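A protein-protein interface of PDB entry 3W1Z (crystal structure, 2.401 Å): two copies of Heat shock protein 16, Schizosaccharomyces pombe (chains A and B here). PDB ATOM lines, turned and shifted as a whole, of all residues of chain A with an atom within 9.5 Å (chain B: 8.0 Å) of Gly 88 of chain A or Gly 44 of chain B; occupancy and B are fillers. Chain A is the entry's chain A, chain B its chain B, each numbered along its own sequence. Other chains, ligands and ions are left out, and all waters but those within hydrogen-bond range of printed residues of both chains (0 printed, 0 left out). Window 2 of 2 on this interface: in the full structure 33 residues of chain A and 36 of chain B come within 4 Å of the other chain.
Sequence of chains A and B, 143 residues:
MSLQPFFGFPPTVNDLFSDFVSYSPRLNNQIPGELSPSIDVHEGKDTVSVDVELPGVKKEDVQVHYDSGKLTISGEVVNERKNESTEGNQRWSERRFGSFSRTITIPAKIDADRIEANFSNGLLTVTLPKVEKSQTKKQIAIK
The guanidinium group (NH2) of Arg 81 of chain A sits close to the side-chain hydroxyl (OG) of Ser 49 of chain B (3.4 Å). The backbone carbonyl oxygen (O) of Asn 89 of chain A lies within hydrogen-bond range of the backbone NH (N) of Glu 43 of chain B, at 3.1 Å. The side-chain amide nitrogen (NE2) of Gln 90 of chain A is in hydrogen-bond range of a ring nitrogen (NE2) of His 42 of chain B. O of Val 41 of chain B lies within hydrogen-bond range of N of Arg 91 of chain A, 2.9 Å away. OE1 of Glu 43 of chain B lies within salt-bridge range of NH1 of Arg 91 of chain A (3.3 Å).
Printed residues of chain B within 4 Å of Arg 81 of chain A: His 42 (3.2 Å) and Ser 49 (3.3 Å). Gly 88 of chain A touches just these residues of chain B: Glu 43 and Gly 44. Of the printed residues of chain B, Arg 91 of chain A touches Val 41 (2.9 Å) and Glu 43 (3.1 Å). Of the printed residues of chain A, His 42 of chain B touches Arg 81, Asn 89 and Gln 90. Of the printed residues of chain A, Glu 43 of chain B touches Gly 88, Asn 89 and Arg 91. Gly 44 of chain B touches one residue of chain A. Lys 130 of chain B touches none of the printed residues of chain A. The nearest residue of chain B that does not touch Gly 88 of chain A is Lys 45 of chain B (5.3 Å).
Hydrophobic or aromatic side chains of chain B that line the printed part of chain A: His 42. Among the printed residues, 10 pairs touch across the chains. Among the printed residues, Asp or Glu carboxylates within 4 Å of a Lys or Arg side-chain nitrogen of the other chain: Arg 91 of chain A with Glu 43 of chain B (3.3 Å).
Arg 81 of chain A touches His 42 of chain B (CG to NE2, 3.2 Å). Glu 43 of chain B touches Gly 88 of chain A. Gly 44 of chain B touches Gly 88 of chain A (CA to CA, 3.97 Å). O of Asn 89 of chain A touches CA of His 42 of chain B, 3.5 Å away. CA of Gln 90 of chain A touches O of Val 41 of chain B (3.7 Å).
No position is printed for both chains. Of the 10 pairs that touch across the chains among the printed residues, none has its exchanged pair printed and touching as well.
The side-chain amide oxygen of Asn 83 of chain A sits close to the backbone carbonyl oxygen of Arg 81 of chain A. The backbone carbonyl oxygen of His 42 of chain B sits at hydrogen-bond distance from the backbone NH of Ser 49 of chain B, 2.9 Å away. OE2 of Glu 43 of chain B lies within salt-bridge range of NZ of Lys 130 of chain B (2.8 Å). NZ of Lys 130 of chain B is in hydrogen-bond range of O of Gly 44 of chain B (2.4 Å).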
ATOM      1  N   ARG A  81     -24.818 -16.541  -7.791  1.00  0.00           N
ATOM      2  CA  ARG A  81     -25.466 -15.257  -7.559  1.00  0.00           C
ATOM      3  C   ARG A  81     -26.244 -15.364  -6.258  1.00  0.00           C
ATOM      4  O   ARG A  81     -26.917 -14.412  -5.846  1.00  0.00           O
ATOM      5  CB  ARG A  81     -26.432 -14.894  -8.691  1.00  0.00           C
ATOM      6  CG  ARG A  81     -25.874 -15.099 -10.099  1.00  0.00           C
ATOM      7  CD  ARG A  81     -24.934 -13.990 -10.533  1.00  0.00           C
ATOM      8  NE  ARG A  81     -24.472 -14.156 -11.915  1.00  0.00           N
ATOM      9  CZ  ARG A  81     -23.464 -13.481 -12.460  1.00  0.00           C
ATOM     10  NH1 ARG A  81     -22.798 -12.595 -11.740  1.00  0.00           N
ATOM     11  NH2 ARG A  81     -23.111 -13.699 -13.719  1.00  0.00           N
ATOM     12  N   LYS A  82     -26.148 -16.524  -5.608  1.00  0.00           N
ATOM     13  CA  LYS A  82     -26.858 -16.777  -4.351  1.00  0.00           C
ATOM     14  C   LYS A  82     -26.039 -16.227  -3.179  1.00  0.00           C
ATOM     15  O   LYS A  82     -26.438 -16.343  -2.020  1.00  0.00           O
ATOM     16  CB  LYS A  82     -27.131 -18.272  -4.165  1.00  0.00           C
ATOM     17  CG  LYS A  82     -26.061 -19.056  -3.408  1.00  0.00           C
ATOM     18  CD  LYS A  82     -26.575 -19.483  -2.044  1.00  0.00           C
ATOM     19  CE  LYS A  82     -25.450 -19.926  -1.135  1.00  0.00           C
ATOM     20  NZ  LYS A  82     -24.377 -18.898  -1.013  1.00  0.00           N
ATOM     21  N   ASN A  83     -24.924 -15.567  -3.498  1.00  0.00           N
ATOM     22  CA  ASN A  83     -23.999 -15.054  -2.487  1.00  0.00           C
ATOM     23  C   ASN A  83     -24.620 -14.062  -1.497  1.00  0.00           C
ATOM     24  O   ASN A  83     -23.996 -13.723  -0.489  1.00  0.00           O
ATOM     25  CB  ASN A  83     -22.733 -14.471  -3.135  1.00  0.00           C
ATOM     26  CG  ASN A  83     -23.004 -13.214  -3.938  1.00  0.00           C
ATOM     27  OD1 ASN A  83     -24.131 -12.959  -4.362  1.00  0.00           O
ATOM     28  ND2 ASN A  83     -21.959 -12.427  -4.163  1.00  0.00           N
ATOM     29  N   GLU A  84     -25.832 -13.592  -1.786  1.00  0.00           N
ATOM     30  CA  GLU A  84     -26.605 -12.829  -0.805  1.00  0.00           C
ATOM     31  C   GLU A  84     -28.113 -12.899  -1.061  1.00  0.00           C
ATOM     32  O   GLU A  84     -28.544 -13.282  -2.146  1.00  0.00           O
ATOM     33  CB  GLU A  84     -26.133 -11.379  -0.737  1.00  0.00           C
ATOM     34  CG  GLU A  84     -26.063 -10.844   0.682  1.00  0.00           C
ATOM     35  CD  GLU A  84     -27.119  -9.802   0.965  1.00  0.00           C
ATOM     36  OE1 GLU A  84     -27.177  -8.803   0.218  1.00  0.00           O
ATOM     37  OE2 GLU A  84     -27.891  -9.983   1.932  1.00  0.00           O
ATOM     38  N   SER A  85     -28.908 -12.530  -0.060  1.00  0.00           N
ATOM     39  CA  SER A  85     -30.366 -12.644  -0.151  1.00  0.00           C
ATOM     40  C   SER A  85     -30.994 -11.415  -0.818  1.00  0.00           C
ATOM     41  O   SER A  85     -32.215 -11.310  -0.942  1.00  0.00           O
ATOM     42  CB  SER A  85     -30.964 -12.840   1.246  1.00  0.00           C
ATOM     43  OG  SER A  85     -30.346 -13.925   1.924  1.00  0.00           O
ATOM     44  N   THR A  86     -30.134 -10.480  -1.210  1.00  0.00           N
ATOM     45  CA  THR A  86     -30.514  -9.179  -1.765  1.00  0.00           C
ATOM     46  C   THR A  86     -29.362  -8.671  -2.626  1.00  0.00           C
ATOM     47  O   THR A  86     -28.526  -9.470  -3.049  1.00  0.00           O
ATOM     48  CB  THR A  86     -30.909  -8.140  -0.687  1.00  0.00           C
ATOM     49  OG1 THR A  86     -30.426  -6.845  -1.063  1.00  0.00           O
ATOM     50  CG2 THR A  86     -30.357  -8.509   0.682  1.00  0.00           C
ATOM     51  N   GLU A  87     -29.328  -7.365  -2.901  1.00  0.00           N
ATOM     52  CA  GLU A  87     -28.299  -6.763  -3.765  1.00  0.00           C
ATOM     53  C   GLU A  87     -28.398  -7.202  -5.225  1.00  0.00           C
ATOM     54  O   GLU A  87     -27.657  -8.059  -5.703  1.00  0.00           O
ATOM     55  CB  GLU A  87     -26.886  -7.015  -3.206  1.00  0.00           C
ATOM     56  CG  GLU A  87     -25.743  -6.446  -4.039  1.00  0.00           C
ATOM     57  CD  GLU A  87     -24.973  -7.520  -4.801  1.00  0.00           C
ATOM     58  OE1 GLU A  87     -25.196  -8.724  -4.544  1.00  0.00           O
ATOM     59  OE2 GLU A  87     -24.142  -7.156  -5.660  1.00  0.00           O
ATOM     60  N   GLY A  88     -29.387  -6.646  -5.911  1.00  0.00           N
ATOM     61  CA  GLY A  88     -29.594  -6.935  -7.313  1.00  0.00           C
ATOM     62  C   GLY A  88     -30.458  -8.167  -7.391  1.00  0.00           C
ATOM     63  O   GLY A  88     -30.384  -9.039  -6.527  1.00  0.00           O
ATOM     64  N   ASN A  89     -31.277  -8.253  -8.427  1.00  0.00           N
ATOM     65  CA  ASN A  89     -32.263  -9.317  -8.496  1.00  0.00           C
ATOM     66  C   ASN A  89     -32.096 -10.191  -9.724  1.00  0.00           C
ATOM     67  O   ASN A  89     -31.483  -9.782 -10.711  1.00  0.00           O
ATOM     68  CB  ASN A  89     -33.679  -8.736  -8.463  1.00  0.00           C
ATOM     69  CG  ASN A  89     -34.016  -8.085  -7.134  1.00  0.00           C
ATOM     70  OD1 ASN A  89     -33.148  -7.536  -6.455  1.00  0.00           O
ATOM     71  ND2 ASN A  89     -35.286  -8.145  -6.755  1.00  0.00           N
ATOM     72  N   GLN A  90     -32.642 -11.399  -9.658  1.00  0.00           N
ATOM     73  CA  GLN A  90     -32.734 -12.221 -10.845  1.00  0.00           C
ATOM     74  C   GLN A  90     -33.918 -11.694 -11.628  1.00  0.00           C
ATOM     75  O   GLN A  90     -35.051 -11.740 -11.152  1.00  0.00           O
ATOM     76  CB  GLN A  90     -33.004 -13.680 -10.479  1.00  0.00           C
ATOM     77  CG  GLN A  90     -31.901 -14.367  -9.704  1.00  0.00           C
ATOM     78  CD  GLN A  90     -31.913 -15.869  -9.910  1.00  0.00           C
ATOM     79  OE1 GLN A  90     -32.918 -16.438 -10.337  1.00  0.00           O
ATOM     80  NE2 GLN A  90     -30.792 -16.517  -9.621  1.00  0.00           N
ATOM     81  N   ARG A  91     -33.659 -11.182 -12.823  1.00  0.00           N
ATOM     82  CA  ARG A  91     -34.742 -10.769 -13.699  1.00  0.00           C
ATOM     83  C   ARG A  91     -35.287 -11.982 -14.439  1.00  0.00           C
ATOM     84  O   ARG A  91     -36.465 -12.037 -14.784  1.00  0.00           O
ATOM     85  CB  ARG A  91     -34.284  -9.686 -14.675  1.00  0.00           C
ATOM     86  CG  ARG A  91     -33.759  -8.431 -13.995  1.00  0.00           C
ATOM     87  CD  ARG A  91     -34.114  -7.178 -14.782  1.00  0.00           C
ATOM     88  NE  ARG A  91     -35.523  -6.817 -14.637  1.00  0.00           N
ATOM     89  CZ  ARG A  91     -36.012  -6.112 -13.620  1.00  0.00           C
ATOM     90  NH1 ARG A  91     -35.211  -5.695 -12.650  1.00  0.00           N
ATOM     91  NH2 ARG A  91     -37.307  -5.827 -13.571  1.00  0.00           N
ATOM     92  N   VAL B  41     -30.479 -14.075 -16.189  1.00  0.00           N
ATOM     93  CA  VAL B  41     -30.187 -12.651 -16.282  1.00  0.00           C
ATOM     94  C   VAL B  41     -30.273 -11.998 -14.909  1.00  0.00           C
ATOM     95  O   VAL B  41     -31.288 -12.112 -14.221  1.00  0.00           O
ATOM     96  CB  VAL B  41     -31.139 -11.929 -17.252  1.00  0.00           C
ATOM     97  CG1 VAL B  41     -30.730 -10.471 -17.402  1.00  0.00           C
ATOM     98  CG2 VAL B  41     -31.145 -12.621 -18.603  1.00  0.00           C
ATOM     99  N   HIS B  42     -29.199 -11.324 -14.511  1.00  0.00           N
ATOM    100  CA  HIS B  42     -29.170 -10.624 -13.234  1.00  0.00           C
ATOM    101  C   HIS B  42     -28.888  -9.146 -13.442  1.00  0.00           C
ATOM    102  O   HIS B  42     -28.086  -8.775 -14.297  1.00  0.00           O
ATOM    103  CB  HIS B  42     -28.112 -11.227 -12.311  1.00  0.00           C
ATOM    104  CG  HIS B  42     -28.407 -12.639 -11.896  1.00  0.00           C
ATOM    105  ND1 HIS B  42     -28.284 -13.701 -12.754  1.00  0.00           N
ATOM    106  CD2 HIS B  42     -28.823 -13.142 -10.710  1.00  0.00           C
ATOM    107  CE1 HIS B  42     -28.614 -14.818 -12.113  1.00  0.00           C
ATOM    108  NE2 HIS B  42     -28.942 -14.504 -10.879  1.00  0.00           N
ATOM    109  N   GLU B  43     -29.551  -8.301 -12.662  1.00  0.00           N
ATOM    110  CA  GLU B  43     -29.318  -6.869 -12.752  1.00  0.00           C
ATOM    111  C   GLU B  43     -29.095  -6.235 -11.387  1.00  0.00           C
ATOM    112  O   GLU B  43     -29.986  -6.233 -10.537  1.00  0.00           O
ATOM    113  CB  GLU B  43     -30.482  -6.169 -13.460  1.00  0.00           C
ATOM    114  CG  GLU B  43     -30.205  -4.706 -13.773  1.00  0.00           C
ATOM    115  CD  GLU B  43     -31.454  -3.931 -14.142  1.00  0.00           C
ATOM    116  OE1 GLU B  43     -32.552  -4.523 -14.126  1.00  0.00           O
ATOM    117  OE2 GLU B  43     -31.338  -2.725 -14.445  1.00  0.00           O
ATOM    118  N   GLY B  44     -27.897  -5.702 -11.182  1.00  0.00           N
ATOM    119  CA  GLY B  44     -27.641  -4.832 -10.053  1.00  0.00           C
ATOM    120  C   GLY B  44     -27.943  -3.430 -10.534  1.00  0.00           C
ATOM    121  O   GLY B  44     -28.185  -3.231 -11.724  1.00  0.00           O
ATOM    122  N   LYS B  45     -27.911  -2.449  -9.639  1.00  0.00           N
ATOM    123  CA  LYS B  45     -28.177  -1.069 -10.034  1.00  0.00           C
ATOM    124  C   LYS B  45     -27.007  -0.520 -10.855  1.00  0.00           C
ATOM    125  O   LYS B  45     -27.078   0.573 -11.415  1.00  0.00           O
ATOM    126  CB  LYS B  45     -28.443  -0.193  -8.806  1.00  0.00           C
ATOM    127  CG  LYS B  45     -29.079   1.155  -9.128  1.00  0.00           C
ATOM    128  CD  LYS B  45     -29.495   1.910  -7.874  1.00  0.00           C
ATOM    129  CE  LYS B  45     -30.961   1.682  -7.529  1.00  0.00           C
ATOM    130  NZ  LYS B  45     -31.246   0.280  -7.118  1.00  0.00           N
ATOM    131  N   ASP B  46     -25.942  -1.311 -10.945  1.00  0.00           N
ATOM    132  CA  ASP B  46     -24.725  -0.907 -11.638  1.00  0.00           C
ATOM    133  C   ASP B  46     -24.502  -1.647 -12.962  1.00  0.00           C
ATOM    134  O   ASP B  46     -24.436  -1.021 -14.016  1.00  0.00           O
ATOM    135  CB  ASP B  46     -23.522  -1.040 -10.709  1.00  0.00           C
ATOM    136  CG  ASP B  46     -23.626  -0.131  -9.499  1.00  0.00           C
ATOM    137  OD1 ASP B  46     -23.103   1.002  -9.558  1.00  0.00           O
ATOM    138  OD2 ASP B  46     -24.248  -0.542  -8.498  1.00  0.00           O
ATOM    139  N   THR B  47     -24.355  -2.968 -12.909  1.00  0.00           N
ATOM    140  CA  THR B  47     -24.176  -3.754 -14.132  1.00  0.00           C
ATOM    141  C   THR B  47     -25.337  -4.709 -14.395  1.00  0.00           C
ATOM    142  O   THR B  47     -26.273  -4.805 -13.600  1.00  0.00           O
ATOM    143  CB  THR B  47     -22.880  -4.588 -14.087  1.00  0.00           C
ATOM    144  OG1 THR B  47     -22.879  -5.411 -12.913  1.00  0.00           O
ATOM    145  CG2 THR B  47     -21.659  -3.688 -14.070  1.00  0.00           C
ATOM    146  N   VAL B  48     -25.264  -5.411 -15.521  1.00  0.00           N
ATOM    147  CA  VAL B  48     -26.182  -6.508 -15.812  1.00  0.00           C
ATOM    148  C   VAL B  48     -25.411  -7.699 -16.378  1.00  0.00           C
ATOM    149  O   VAL B  48     -24.667  -7.570 -17.354  1.00  0.00           O
ATOM    150  CB  VAL B  48     -27.334  -6.094 -16.764  1.00  0.00           C
ATOM    151  CG1 VAL B  48     -26.807  -5.332 -17.967  1.00  0.00           C
ATOM    152  CG2 VAL B  48     -28.130  -7.315 -17.206  1.00  0.00           C
ATOM    153  N   SER B  49     -25.582  -8.855 -15.745  1.00  0.00           N
ATOM    154  CA  SER B  49     -24.850 -10.055 -16.128  1.00  0.00           C
ATOM    155  C   SER B  49     -25.764 -11.108 -16.744  1.00  0.00           C
ATOM    156  O   SER B  49     -26.871 -11.350 -16.258  1.00  0.00           O
ATOM    157  CB  SER B  49     -24.122 -10.639 -14.916  1.00  0.00           C
ATOM    158  OG  SER B  49     -25.033 -10.946 -13.874  1.00  0.00           O
ATOM    159  N   ALA B 108     -31.961  -1.683 -20.539  1.00  0.00           N
ATOM    160  CA  ALA B 108     -31.160  -0.726 -19.790  1.00  0.00           C
ATOM    161  C   ALA B 108     -30.165  -0.027 -20.704  1.00  0.00           C
ATOM    162  O   ALA B 108     -29.827  -0.535 -21.773  1.00  0.00           O
ATOM    163  CB  ALA B 108     -30.433  -1.420 -18.648  1.00  0.00           C
ATOM    164  N   LEU B 128     -22.579  -6.355 -18.982  1.00  0.00           N
ATOM    165  CA  LEU B 128     -22.877  -5.063 -19.585  1.00  0.00           C
ATOM    166  C   LEU B 128     -23.036  -3.998 -18.503  1.00  0.00           C
ATOM    167  O   LEU B 128     -24.001  -4.020 -17.741  1.00  0.00           O
ATOM    168  CB  LEU B 128     -24.145  -5.140 -20.443  1.00  0.00           C
ATOM    169  CG  LEU B 128     -24.233  -6.234 -21.514  1.00  0.00           C
ATOM    170  CD1 LEU B 128     -24.823  -7.522 -20.950  1.00  0.00           C
ATOM    171  CD2 LEU B 128     -25.041  -5.755 -22.710  1.00  0.00           C
ATOM    172  N   LYS B 130     -24.032  -0.623 -16.759  1.00  0.00           N
ATOM    173  CA  LYS B 130     -25.076   0.368 -16.992  1.00  0.00           C
ATOM    174  C   LYS B 130     -24.598   1.769 -16.647  1.00  0.00           C
ATOM    175  O   LYS B 130     -23.933   1.981 -15.633  1.00  0.00           O
ATOM    176  CB  LYS B 130     -26.336   0.053 -16.183  1.00  0.00           C
ATOM    177  CG  LYS B 130     -27.034  -1.238 -16.563  1.00  0.00           C
ATOM    178  CD  LYS B 130     -28.257  -1.458 -15.689  1.00  0.00           C
ATOM    179  CE  LYS B 130     -27.897  -1.345 -14.218  1.00  0.00           C
ATOM    180  NZ  LYS B 130     -29.055  -1.632 -13.328  1.00  0.00           N
